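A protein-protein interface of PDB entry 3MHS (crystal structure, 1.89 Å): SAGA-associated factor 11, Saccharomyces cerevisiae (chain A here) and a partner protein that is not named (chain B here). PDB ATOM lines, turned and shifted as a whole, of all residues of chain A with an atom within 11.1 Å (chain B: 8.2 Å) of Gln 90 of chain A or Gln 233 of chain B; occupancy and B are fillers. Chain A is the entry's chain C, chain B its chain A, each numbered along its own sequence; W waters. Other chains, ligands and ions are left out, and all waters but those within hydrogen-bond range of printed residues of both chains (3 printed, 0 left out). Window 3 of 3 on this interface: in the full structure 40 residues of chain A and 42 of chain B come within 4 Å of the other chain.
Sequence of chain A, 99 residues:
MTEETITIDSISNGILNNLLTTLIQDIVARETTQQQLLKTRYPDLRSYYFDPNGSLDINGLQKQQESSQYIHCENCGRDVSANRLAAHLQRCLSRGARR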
ATOM      1  N   CYS A  73      20.794 -29.830  13.165  1.00  0.00           N
ATOM      2  CA  CYS A  73      20.808 -28.680  12.252  1.00  0.00           C
ATOM      3  C   CYS A  73      19.470 -28.681  11.507  1.00  0.00           C
ATOM      4  O   CYS A  73      19.177 -29.580  10.779  1.00  0.00           O
ATOM      5  CB  CYS A  73      22.026 -28.748  11.273  1.00  0.00           C
ATOM      6  SG  CYS A  73      22.122 -27.520   9.852  1.00  0.00           S
ATOM      7  N   ASN A  75      18.737 -26.852   9.075  1.00  0.00           N
ATOM      8  CA  ASN A  75      18.966 -26.621   7.630  1.00  0.00           C
ATOM      9  C   ASN A  75      19.210 -27.877   6.806  1.00  0.00           C
ATOM     10  O   ASN A  75      18.778 -27.940   5.649  1.00  0.00           O
ATOM     11  CB  ASN A  75      20.095 -25.579   7.374  1.00  0.00           C
ATOM     12  CG  ASN A  75      20.103 -25.055   5.914  1.00  0.00           C
ATOM     13  OD1 ASN A  75      19.107 -24.540   5.440  1.00  0.00           O
ATOM     14  ND2 ASN A  75      21.224 -25.213   5.211  1.00  0.00           N
ATOM     15  N   CYS A  76      19.848 -28.893   7.388  1.00  0.00           N
ATOM     16  CA  CYS A  76      20.200 -30.114   6.656  1.00  0.00           C
ATOM     17  C   CYS A  76      19.737 -31.420   7.338  1.00  0.00           C
ATOM     18  O   CYS A  76      19.887 -32.495   6.770  1.00  0.00           O
ATOM     19  CB  CYS A  76      21.716 -30.158   6.449  1.00  0.00           C
ATOM     20  SG  CYS A  76      22.651 -30.489   7.942  1.00  0.00           S
ATOM     21  N   ARG A  78      21.075 -32.980  10.000  1.00  0.00           N
ATOM     22  CA  ARG A  78      22.105 -33.805  10.627  1.00  0.00           C
ATOM     23  C   ARG A  78      22.375 -33.332  12.045  1.00  0.00           C
ATOM     24  O   ARG A  78      22.216 -32.143  12.365  1.00  0.00           O
ATOM     25  CB  ARG A  78      23.403 -33.777   9.815  1.00  0.00           C
ATOM     26  CG  ARG A  78      23.258 -34.251   8.360  1.00  0.00           C
ATOM     27  CD  ARG A  78      24.505 -33.886   7.565  1.00  0.00           C
ATOM     28  NE  ARG A  78      24.278 -33.943   6.129  1.00  0.00           N
ATOM     29  CZ  ARG A  78      24.357 -32.902   5.317  1.00  0.00           C
ATOM     30  NH1 ARG A  78      24.703 -31.704   5.791  1.00  0.00           N
ATOM     31  NH2 ARG A  78      24.127 -33.075   4.024  1.00  0.00           N
ATOM     32  N   VAL A  80      25.139 -32.372  14.652  1.00  0.00           N
ATOM     33  CA  VAL A  80      26.419 -31.718  14.583  1.00  0.00           C
ATOM     34  C   VAL A  80      26.935 -31.483  16.001  1.00  0.00           C
ATOM     35  O   VAL A  80      26.143 -31.089  16.876  1.00  0.00           O
ATOM     36  CB  VAL A  80      26.230 -30.336  13.852  1.00  0.00           C
ATOM     37  CG1 VAL A  80      27.474 -29.511  13.887  1.00  0.00           C
ATOM     38  CG2 VAL A  80      25.766 -30.584  12.371  1.00  0.00           C
ATOM     39  N   SER A  81      28.229 -31.747  16.243  1.00  0.00           N
ATOM     40  CA  SER A  81      28.831 -31.512  17.554  1.00  0.00           C
ATOM     41  C   SER A  81      28.656 -30.013  17.840  1.00  0.00           C
ATOM     42  O   SER A  81      28.928 -29.169  16.977  1.00  0.00           O
ATOM     43  CB  SER A  81      30.311 -31.872  17.570  1.00  0.00           C
ATOM     44  OG  SER A  81      30.500 -33.237  17.267  1.00  0.00           O
ATOM     45  N   ASN A  83      30.169 -27.821  19.541  1.00  0.00           N
ATOM     46  CA  ASN A  83      31.348 -26.948  19.454  1.00  0.00           C
ATOM     47  C   ASN A  83      31.878 -26.788  18.025  1.00  0.00           C
ATOM     48  O   ASN A  83      32.888 -26.119  17.781  1.00  0.00           O
ATOM     49  CB  ASN A  83      32.450 -27.348  20.484  1.00  0.00           C
ATOM     50  CG  ASN A  83      33.059 -28.710  20.206  1.00  0.00           C
ATOM     51  OD1 ASN A  83      32.713 -29.371  19.226  1.00  0.00           O
ATOM     52  ND2 ASN A  83      33.965 -29.146  21.085  1.00  0.00           N
ATOM     53  N   ARG A  84      31.158 -27.354  17.054  1.00  0.00           N
ATOM     54  CA  ARG A  84      31.545 -27.213  15.671  1.00  0.00           C
ATOM     55  C   ARG A  84      30.401 -26.680  14.840  1.00  0.00           C
ATOM     56  O   ARG A  84      30.427 -26.780  13.607  1.00  0.00           O
ATOM     57  CB  ARG A  84      31.975 -28.569  15.115  1.00  0.00           C
ATOM     58  CG  ARG A  84      33.342 -29.045  15.622  1.00  0.00           C
ATOM     59  CD  ARG A  84      34.497 -28.194  15.092  1.00  0.00           C
ATOM     60  NE  ARG A  84      34.650 -28.291  13.654  1.00  0.00           N
ATOM     61  CZ  ARG A  84      35.669 -27.787  12.972  1.00  0.00           C
ATOM     62  NH1 ARG A  84      36.622 -27.124  13.599  1.00  0.00           N
ATOM     63  NH2 ARG A  84      35.736 -27.946  11.663  1.00  0.00           N
ATOM     64  N   LEU A  85      29.361 -26.134  15.482  1.00  0.00           N
ATOM     65  CA  LEU A  85      28.209 -25.685  14.711  1.00  0.00           C
ATOM     66  C   LEU A  85      28.567 -24.546  13.783  1.00  0.00           C
ATOM     67  O   LEU A  85      28.084 -24.487  12.647  1.00  0.00           O
ATOM     68  CB  LEU A  85      27.066 -25.297  15.622  1.00  0.00           C
ATOM     69  CG  LEU A  85      25.615 -25.221  15.156  1.00  0.00           C
ATOM     70  CD1 LEU A  85      25.021 -23.908  15.230  1.00  0.00           C
ATOM     71  CD2 LEU A  85      25.241 -25.998  13.871  1.00  0.00           C
ATOM     72  N   ALA A  86      29.396 -23.609  14.251  1.00  0.00           N
ATOM     73  CA  ALA A  86      29.745 -22.484  13.408  1.00  0.00           C
ATOM     74  C   ALA A  86      30.478 -22.957  12.134  1.00  0.00           C
ATOM     75  O   ALA A  86      30.167 -22.504  11.039  1.00  0.00           O
ATOM     76  CB  ALA A  86      30.562 -21.400  14.207  1.00  0.00           C
ATOM     77  N   ALA A  87      31.379 -23.914  12.286  1.00  0.00           N
ATOM     78  CA  ALA A  87      32.118 -24.523  11.177  1.00  0.00           C
ATOM     79  C   ALA A  87      31.142 -25.199  10.234  1.00  0.00           C
ATOM     80  O   ALA A  87      31.239 -25.050   9.021  1.00  0.00           O
ATOM     81  CB  ALA A  87      33.159 -25.550  11.705  1.00  0.00           C
ATOM     82  N   HIS A  88      30.196 -25.957  10.793  1.00  0.00           N
ATOM     83  CA  HIS A  88      29.183 -26.638  10.003  1.00  0.00           C
ATOM     84  C   HIS A  88      28.327 -25.638   9.190  1.00  0.00           C
ATOM     85  O   HIS A  88      28.041 -25.831   8.002  1.00  0.00           O
ATOM     86  CB  HIS A  88      28.228 -27.449  10.895  1.00  0.00           C
ATOM     87  CG  HIS A  88      27.109 -28.070  10.122  1.00  0.00           C
ATOM     88  ND1 HIS A  88      27.333 -29.093   9.232  1.00  0.00           N
ATOM     89  CD2 HIS A  88      25.799 -27.742   9.999  1.00  0.00           C
ATOM     90  CE1 HIS A  88      26.195 -29.421   8.647  1.00  0.00           C
ATOM     91  NE2 HIS A  88      25.246 -28.618   9.098  1.00  0.00           N
ATOM     92  N   LEU A  89      27.901 -24.562   9.829  1.00  0.00           N
ATOM     93  CA  LEU A  89      27.018 -23.609   9.151  1.00  0.00           C
ATOM     94  C   LEU A  89      27.715 -22.987   7.926  1.00  0.00           C
ATOM     95  O   LEU A  89      27.060 -22.721   6.943  1.00  0.00           O
ATOM     96  CB  LEU A  89      26.526 -22.524  10.110  1.00  0.00           C
ATOM     97  CG  LEU A  89      25.600 -22.950  11.256  1.00  0.00           C
ATOM     98  CD1 LEU A  89      25.242 -21.777  12.144  1.00  0.00           C
ATOM     99  CD2 LEU A  89      24.342 -23.606  10.767  1.00  0.00           C
ATOM    100  N   GLN A  90      29.034 -22.798   7.995  1.00  0.00           N
ATOM    101  CA  GLN A  90      29.841 -22.277   6.869  1.00  0.00           C
ATOM    102  C   GLN A  90      29.737 -23.205   5.655  1.00  0.00           C
ATOM    103  O   GLN A  90      29.846 -22.747   4.508  1.00  0.00           O
ATOM    104  CB  GLN A  90      31.327 -22.258   7.219  1.00  0.00           C
ATOM    105  CG  GLN A  90      31.818 -21.130   8.090  1.00  0.00           C
ATOM    106  CD  GLN A  90      33.322 -21.022   8.015  1.00  0.00           C
ATOM    107  OE1 GLN A  90      33.995 -21.982   7.641  1.00  0.00           O
ATOM    108  NE2 GLN A  90      33.863 -19.843   8.347  1.00  0.00           N
ATOM    109  N   ARG A  91      29.663 -24.515   5.927  1.00  0.00           N
ATOM    110  CA  ARG A  91      29.556 -25.517   4.863  1.00  0.00           C
ATOM    111  C   ARG A  91      28.108 -25.872   4.550  1.00  0.00           C
ATOM    112  O   ARG A  91      27.891 -26.622   3.632  1.00  0.00           O
ATOM    113  CB  ARG A  91      30.202 -26.870   5.241  1.00  0.00           C
ATOM    114  CG  ARG A  91      31.571 -26.891   5.738  1.00  0.00           C
ATOM    115  CD  ARG A  91      31.951 -28.297   6.233  1.00  0.00           C
ATOM    116  NE  ARG A  91      32.045 -29.252   5.115  1.00  0.00           N
ATOM    117  CZ  ARG A  91      31.241 -30.293   4.930  1.00  0.00           C
ATOM    118  NH1 ARG A  91      30.331 -30.642   5.849  1.00  0.00           N
ATOM    119  NH2 ARG A  91      31.393 -31.050   3.854  1.00  0.00           N
ATOM    120  N   CYS A  92      27.146 -25.459   5.369  1.00  0.00           N
ATOM    121  CA  CYS A  92      25.741 -25.894   5.257  1.00  0.00           C
ATOM    122  C   CYS A  92      24.807 -24.786   4.765  1.00  0.00           C
ATOM    123  O   CYS A  92      23.962 -25.036   3.917  1.00  0.00           O
ATOM    124  CB  CYS A  92      25.208 -26.426   6.593  1.00  0.00           C
ATOM    125  SG  CYS A  92      23.522 -27.051   6.466  1.00  0.00           S
ATOM    126  N   LEU A  93      25.012 -23.553   5.225  1.00  0.00           N
ATOM    127  CA  LEU A  93      24.124 -22.445   4.837  1.00  0.00           C
ATOM    128  C   LEU A  93      24.403 -21.907   3.399  1.00  0.00           C
ATOM    129  O   LEU A  93      23.647 -21.109   2.871  1.00  0.00           O
ATOM    130  CB  LEU A  93      24.244 -21.311   5.835  1.00  0.00           C
ATOM    131  CG  LEU A  93      23.822 -21.577   7.290  1.00  0.00           C
ATOM    132  CD1 LEU A  93      24.098 -20.410   8.201  1.00  0.00           C
ATOM    133  CD2 LEU A  93      22.375 -21.975   7.343  1.00  0.00           C
ATOM    134  N   SER A  94      25.519 -22.308   2.812  1.00  0.00           N
ATOM    135  CA  SER A  94      25.886 -21.802   1.497  1.00  0.00           C
ATOM    136  C   SER A  94      25.196 -22.604   0.407  1.00  0.00           C
ATOM    137  O   SER A  94      24.631 -23.665   0.672  1.00  0.00           O
ATOM    138  CB  SER A  94      27.406 -21.849   1.327  1.00  0.00           C
ATOM    139  OG  SER A  94      27.779 -21.569   0.001  1.00  0.00           O
ATOM    140  N   ARG A  95      25.234 -22.075  -0.813  1.00  0.00           N
ATOM    141  CA  ARG A  95      24.754 -22.773  -2.034  1.00  0.00           C
ATOM    142  C   ARG A  95      24.233 -21.705  -2.984  1.00  0.00           C
ATOM    143  O   ARG A  95      24.656 -20.551  -2.896  1.00  0.00           O
ATOM    144  CB  ARG A  95      23.686 -23.845  -1.767  1.00  0.00           C
ATOM    145  CG  ARG A  95      23.034 -24.432  -3.015  1.00  0.00           C
ATOM    146  CD  ARG A  95      23.639 -25.789  -3.436  1.00  0.00           C
ATOM    147  NE  ARG A  95      24.591 -25.695  -4.555  1.00  0.00           N
ATOM    148  CZ  ARG A  95      24.317 -25.965  -5.837  1.00  0.00           C
ATOM    149  NH1 ARG A  95      23.096 -26.332  -6.225  1.00  0.00           N
ATOM    150  NH2 ARG A  95      25.277 -25.856  -6.750  1.00  0.00           N
ATOM    151  N   PHE B 152      33.153 -14.192  21.701  1.00  0.00           N
ATOM    152  CA  PHE B 152      33.129 -12.738  21.427  1.00  0.00           C
ATOM    153  C   PHE B 152      31.704 -12.281  21.121  1.00  0.00           C
ATOM    154  O   PHE B 152      31.407 -11.088  21.237  1.00  0.00           O
ATOM    155  CB  PHE B 152      34.110 -12.342  20.305  1.00  0.00           C
ATOM    156  CG  PHE B 152      33.669 -12.801  18.905  1.00  0.00           C
ATOM    157  CD1 PHE B 152      32.844 -11.995  18.147  1.00  0.00           C
ATOM    158  CD2 PHE B 152      34.037 -14.022  18.401  1.00  0.00           C
ATOM    159  CE1 PHE B 152      32.408 -12.402  16.888  1.00  0.00           C
ATOM    160  CE2 PHE B 152      33.589 -14.436  17.163  1.00  0.00           C
ATOM    161  CZ  PHE B 152      32.757 -13.620  16.419  1.00  0.00           C
ATOM    162  N   MET B 153      30.851 -13.241  20.748  1.00  0.00           N
ATOM    163  CA  MET B 153      29.445 -13.006  20.464  1.00  0.00           C
ATOM    164  C   MET B 153      28.618 -13.141  21.726  1.00  0.00           C
ATOM    165  O   MET B 153      27.871 -12.254  22.081  1.00  0.00           O
ATOM    166  CB  MET B 153      28.939 -14.018  19.419  1.00  0.00           C
ATOM    167  CG  MET B 153      29.717 -13.957  18.131  1.00  0.00           C
ATOM    168  SD  MET B 153      29.254 -15.296  16.990  1.00  0.00           S
ATOM    169  CE  MET B 153      27.725 -14.652  16.299  1.00  0.00           C
ATOM    170  N   LEU B 225      23.355 -16.862  15.062  1.00  0.00           N
ATOM    171  CA  LEU B 225      24.562 -17.315  14.334  1.00  0.00           C
ATOM    172  C   LEU B 225      24.250 -17.458  12.850  1.00  0.00           C
ATOM    173  O   LEU B 225      25.097 -17.211  11.979  1.00  0.00           O
ATOM    174  CB  LEU B 225      25.048 -18.664  14.877  1.00  0.00           C
ATOM    175  CG  LEU B 225      26.205 -18.633  15.857  1.00  0.00           C
ATOM    176  CD1 LEU B 225      25.933 -17.780  17.029  1.00  0.00           C
ATOM    177  CD2 LEU B 225      26.631 -20.031  16.278  1.00  0.00           C
ATOM    178  N   CYS B 227      21.760 -15.753  11.146  1.00  0.00           N
ATOM    179  CA  CYS B 227      21.688 -14.370  10.651  1.00  0.00           C
ATOM    180  C   CYS B 227      23.068 -13.757  10.373  1.00  0.00           C
ATOM    181  O   CYS B 227      23.260 -13.102   9.343  1.00  0.00           O
ATOM    182  CB  CYS B 227      20.968 -13.448  11.609  1.00  0.00           C
ATOM    183  SG  CYS B 227      19.244 -13.810  11.802  1.00  0.00           S
ATOM    184  N   ALA B 228      23.999 -13.959  11.312  1.00  0.00           N
ATOM    185  CA  ALA B 228      25.342 -13.408  11.221  1.00  0.00           C
ATOM    186  C   ALA B 228      26.099 -13.957  10.051  1.00  0.00           C
ATOM    187  O   ALA B 228      26.752 -13.185   9.339  1.00  0.00           O
ATOM    188  CB  ALA B 228      26.131 -13.619  12.567  1.00  0.00           C
ATOM    189  N   TRP B 229      26.030 -15.271   9.840  1.00  0.00           N
ATOM    190  CA  TRP B 229      26.718 -15.891   8.741  1.00  0.00           C
ATOM    191  C   TRP B 229      26.279 -15.238   7.428  1.00  0.00           C
ATOM    192  O   TRP B 229      27.105 -14.988   6.571  1.00  0.00           O
ATOM    193  CB  TRP B 229      26.498 -17.406   8.674  1.00  0.00           C
ATOM    194  CG  TRP B 229      27.226 -18.027   7.498  1.00  0.00           C
ATOM    195  CD1 TRP B 229      28.513 -18.451   7.492  1.00  0.00           C
ATOM    196  CD2 TRP B 229      26.739 -18.232   6.170  1.00  0.00           C
ATOM    197  NE1 TRP B 229      28.861 -18.899   6.273  1.00  0.00           N
ATOM    198  CE2 TRP B 229      27.803 -18.769   5.423  1.00  0.00           C
ATOM    199  CE3 TRP B 229      25.534 -17.970   5.528  1.00  0.00           C
ATOM    200  CZ2 TRP B 229      27.693 -19.087   4.080  1.00  0.00           C
ATOM    201  CZ3 TRP B 229      25.412 -18.287   4.176  1.00  0.00           C
ATOM    202  CH2 TRP B 229      26.488 -18.865   3.472  1.00  0.00           C
ATOM    203  N   LYS B 230      24.983 -14.972   7.277  1.00  0.00           N
ATOM    204  CA  LYS B 230      24.457 -14.423   6.009  1.00  0.00           C
ATOM    205  C   LYS B 230      24.944 -12.987   5.737  1.00  0.00           C
ATOM    206  O   LYS B 230      25.161 -12.615   4.604  1.00  0.00           O
ATOM    207  CB  LYS B 230      22.928 -14.454   6.017  1.00  0.00           C
ATOM    208  CG  LYS B 230      22.352 -15.854   6.112  1.00  0.00           C
ATOM    209  CD  LYS B 230      20.824 -15.863   6.254  1.00  0.00           C
ATOM    210  CE  LYS B 230      20.331 -17.309   6.386  1.00  0.00           C
ATOM    211  NZ  LYS B 230      18.864 -17.391   6.682  1.00  0.00           N
ATOM    212  N   ILE B 231      25.166 -12.208   6.775  1.00  0.00           N
ATOM    213  CA  ILE B 231      25.551 -10.803   6.632  1.00  0.00           C
ATOM    214  C   ILE B 231      27.069 -10.609   6.661  1.00  0.00           C
ATOM    215  O   ILE B 231      27.645  -9.848   5.870  1.00  0.00           O
ATOM    216  CB  ILE B 231      24.857  -9.987   7.765  1.00  0.00           C
ATOM    217  CG1 ILE B 231      23.357 -10.045   7.544  1.00  0.00           C
ATOM    218  CG2 ILE B 231      25.334  -8.546   7.798  1.00  0.00           C
ATOM    219  CD1 ILE B 231      22.559 -10.306   8.792  1.00  0.00           C
ATOM    220  N   ASN B 232      27.734 -11.300   7.578  1.00  0.00           N
ATOM    221  CA  ASN B 232      29.196 -11.167   7.750  1.00  0.00           C
ATOM    222  C   ASN B 232      29.787 -12.417   8.343  1.00  0.00           C
ATOM    223  O   ASN B 232      29.890 -12.554   9.557  1.00  0.00           O
ATOM    224  CB  ASN B 232      29.524  -9.972   8.656  1.00  0.00           C
ATOM    225  CG  ASN B 232      31.025  -9.686   8.764  1.00  0.00           C
ATOM    226  OD1 ASN B 232      31.873 -10.469   8.354  1.00  0.00           O
ATOM    227  ND2 ASN B 232      31.344  -8.529   9.310  1.00  0.00           N
ATOM    228  N   GLN B 233      30.263 -13.282   7.473  1.00  0.00           N
ATOM    229  CA  GLN B 233      30.748 -14.581   7.914  1.00  0.00           C
ATOM    230  C   GLN B 233      31.935 -14.453   8.855  1.00  0.00           C
ATOM    231  O   GLN B 233      32.099 -15.297   9.739  1.00  0.00           O
ATOM    232  CB  GLN B 233      31.065 -15.552   6.739  1.00  0.00           C
ATOM    233  CG  GLN B 233      32.479 -15.437   6.147  1.00  0.00           C
ATOM    234  CD  GLN B 233      33.489 -16.451   6.703  1.00  0.00           C
ATOM    235  OE1 GLN B 233      33.306 -17.665   6.577  1.00  0.00           O
ATOM    236  NE2 GLN B 233      34.591 -15.951   7.245  1.00  0.00           N
ATOM    237  N   ASN B 234      32.753 -13.420   8.714  1.00  0.00           N
ATOM    238  CA  ASN B 234      33.875 -13.318   9.618  1.00  0.00           C
ATOM    239  C   ASN B 234      33.460 -13.127  11.073  1.00  0.00           C
ATOM    240  O   ASN B 234      34.227 -13.495  11.938  1.00  0.00           O
ATOM    241  CB  ASN B 234      34.831 -12.194   9.263  1.00  0.00           C
ATOM    242  CG  ASN B 234      35.508 -12.383   7.973  1.00  0.00           C
ATOM    243  OD1 ASN B 234      35.698 -11.402   7.258  1.00  0.00           O
ATOM    244  ND2 ASN B 234      35.839 -13.622   7.615  1.00  0.00           N
ATOM    245  N   LEU B 235      32.290 -12.518  11.333  1.00  0.00           N
ATOM    246  CA  LEU B 235      31.802 -12.242  12.681  1.00  0.00           C
ATOM    247  C   LEU B 235      30.721 -13.226  13.171  1.00  0.00           C
ATOM    248  O   LEU B 235      29.996 -12.936  14.148  1.00  0.00           O
ATOM    249  CB  LEU B 235      31.268 -10.798  12.781  1.00  0.00           C
ATOM    250  CG  LEU B 235      32.281  -9.703  12.517  1.00  0.00           C
ATOM    251  CD1 LEU B 235      31.658  -8.325  12.615  1.00  0.00           C
ATOM    252  CD2 LEU B 235      33.439  -9.828  13.543  1.00  0.00           C
ATOM    253  N   ALA B 236      30.637 -14.387  12.519  1.00  0.00           N
ATOM    254  CA  ALA B 236      29.515 -15.306  12.738  1.00  0.00           C
ATOM    255  C   ALA B 236      29.857 -16.459  13.648  1.00  0.00           C
ATOM    256  O   ALA B 236      28.975 -17.266  13.964  1.00  0.00           O
ATOM    257  CB  ALA B 236      28.956 -15.827  11.401  1.00  0.00           C
ATOM    258  N   GLY B 237      31.134 -16.589  14.028  1.00  0.00           N
ATOM    259  CA  GLY B 237      31.480 -17.457  15.165  1.00  0.00           C
ATOM    260  C   GLY B 237      32.482 -18.552  14.935  1.00  0.00           C
ATOM    261  O   GLY B 237      32.913 -19.200  15.883  1.00  0.00           O
ATOM    262  N   TYR B 238      32.892 -18.759  13.693  1.00  0.00           N
ATOM    263  CA  TYR B 238      33.856 -19.790  13.414  1.00  0.00           C
ATOM    264  C   TYR B 238      35.265 -19.397  13.915  1.00  0.00           C
ATOM    265  O   TYR B 238      36.037 -20.229  14.480  1.00  0.00           O
ATOM    266  CB  TYR B 238      33.905 -20.038  11.919  1.00  0.00           C
ATOM    267  CG  TYR B 238      34.988 -20.986  11.573  1.00  0.00           C
ATOM    268  CD1 TYR B 238      34.967 -22.284  12.050  1.00  0.00           C
ATOM    269  CD2 TYR B 238      36.092 -20.572  10.842  1.00  0.00           C
ATOM    270  CE1 TYR B 238      35.966 -23.166  11.760  1.00  0.00           C
ATOM    271  CE2 TYR B 238      37.125 -21.454  10.564  1.00  0.00           C
ATOM    272  CZ  TYR B 238      37.041 -22.759  11.004  1.00  0.00           C
ATOM    273  OH  TYR B 238      38.049 -23.659  10.728  1.00  0.00           O
ATOM    274  N   SER B 239      35.591 -18.133  13.693  1.00  0.00           N
ATOM    275  CA  SER B 239      36.915 -17.621  13.999  1.00  0.00           C
ATOM    276  C   SER B 239      36.928 -16.631  15.161  1.00  0.00           C
ATOM    277  O   SER B 239      35.938 -15.990  15.442  1.00  0.00           O
ATOM    278  CB  SER B 239      37.516 -16.966  12.745  1.00  0.00           C
ATOM    279  OG  SER B 239      36.795 -15.795  12.357  1.00  0.00           O
ATOM    280  N   GLN B 241      37.440 -13.252  17.071  1.00  0.00           N
ATOM    281  CA  GLN B 241      37.200 -11.885  16.670  1.00  0.00           C
ATOM    282  C   GLN B 241      37.098 -10.969  17.876  1.00  0.00           C
ATOM    283  O   GLN B 241      37.082 -11.427  19.011  1.00  0.00           O
ATOM    284  CB  GLN B 241      35.922 -11.830  15.836  1.00  0.00           C
ATOM    285  CG  GLN B 241      35.950 -12.664  14.546  1.00  0.00           C
ATOM    286  CD  GLN B 241      36.893 -12.155  13.463  1.00  0.00           C
ATOM    287  OE1 GLN B 241      37.217 -10.961  13.381  1.00  0.00           O
ATOM    288  NE2 GLN B 241      37.308 -13.058  12.598  1.00  0.00           N
ATOM    289  N   PHE B 249      28.730  -4.024  15.419  1.00  0.00           N
ATOM    290  CA  PHE B 249      27.999  -4.777  14.399  1.00  0.00           C
ATOM    291  C   PHE B 249      26.545  -5.076  14.758  1.00  0.00           C
ATOM    292  O   PHE B 249      25.663  -4.745  13.974  1.00  0.00           O
ATOM    293  CB  PHE B 249      28.750  -6.069  14.094  1.00  0.00           C
ATOM    294  CG  PHE B 249      28.003  -6.996  13.163  1.00  0.00           C
ATOM    295  CD1 PHE B 249      28.030  -6.789  11.795  1.00  0.00           C
ATOM    296  CD2 PHE B 249      27.356  -8.093  13.661  1.00  0.00           C
ATOM    297  CE1 PHE B 249      27.334  -7.682  10.916  1.00  0.00           C
ATOM    298  CE2 PHE B 249      26.677  -8.996  12.796  1.00  0.00           C
ATOM    299  CZ  PHE B 249      26.692  -8.778  11.443  1.00  0.00           C
HETATM  300  O   HOH W   1      35.727 -17.730   8.563  1.00  0.00           O
HETATM  301  O   HOH W   2      38.945 -25.993  12.591  1.00  0.00           O
HETATM  302  O   HOH W   3      37.545 -26.479  10.200  1.00  0.00           O
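The side-chain amide nitrogen (NE2) of Gln 90 of chain A is in hydrogen-bond range of the side-chain amide oxygen (OE1) of Gln 233 of chain B.
NE2 of Gln 233 of chain B lies close to ND2 of Asn 234 of chain B, 2.7 Å away. The backbone NH (N) of Gly 237 of chain B sits close to the side-chain sulfur (SD) of Met 153 of chain B, 3.7 Å away.
C of Gly 237 of chain B touches CB of Ala 86 of chain A, at 3.5 Å. Ala 86 of chain A touches Tyr 238 of chain B. Tyr 238 of chain B touches Ala 87 of chain A (CE1 to CB, 3.7 Å). Gln 90 of chain A touches Trp 229 of chain B. Gln 90 of chain A touches Tyr 238 of chain B (NE2 to CD2, 3.4 Å). CZ3 of Trp 229 of chain B touches O of Leu 93 of chain A, 3.6 Å away. Ser 94 of chain A touches Trp 229 of chain B (CA to CH2, 3.6 Å).
Of the printed residues of chain B, Gln 90 of chain A touches Trp 229 (3.6 Å), Gln 233 (2.9 Å) and Tyr 238 (3.4 Å). Of the printed residues of chain A, Gln 233 of chain B touches Gln 90. No residue of chain A comes within 4 Å of Ala 236 of chain B. Of the printed residues of chain A, Tyr 238 of chain B touches Ala 86, Ala 87 and Gln 90. Printed residues of chain A within 4 Å of Gly 237 of chain B: Ala 86 (3.5 Å). Printed residues of chain A within 4 Å of Trp 229 of chain B: Gln 90, Leu 93 and Ser 94. Arg 78 of chain A touches none of the printed residues of chain B. The nearest printed residue of chain A that does not touch Trp 229 of chain B is Leu 89 of chain A (4.3 Å).
Hydrophobic or aromatic side chains of chain A within 4 Å of the printed part of chain B: Ala 86, Ala 87 and Leu 93. Of the 18 printed residues of chain B, 4 touch a printed residue of chain A. Hydrophobic or aromatic side chains of chain B that line the printed part of chain A: Trp 229 and Tyr 238. Along chain B the printed residues that touch a printed residue of chain A span positions 229 to 238.
Water W1 lies within hydrogen-bond range of the side-chain amide nitrogen of Gln 233 of chain B (2.5 Å) and the side-chain amide nitrogen of Gln 90 of chain A (2.8 Å). Water W3 lies within hydrogen-bond range of the guanidinium group of Arg 84 of chain A (2.8 Å) and the side-chain hydroxyl of Tyr 238 of chain B (2.9 Å). Water W2 bridges the guanidinium group of Arg 84 of chain A (2.8 Å) and the side-chain hydroxyl of Tyr 238 of chain B (3.1 Å).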
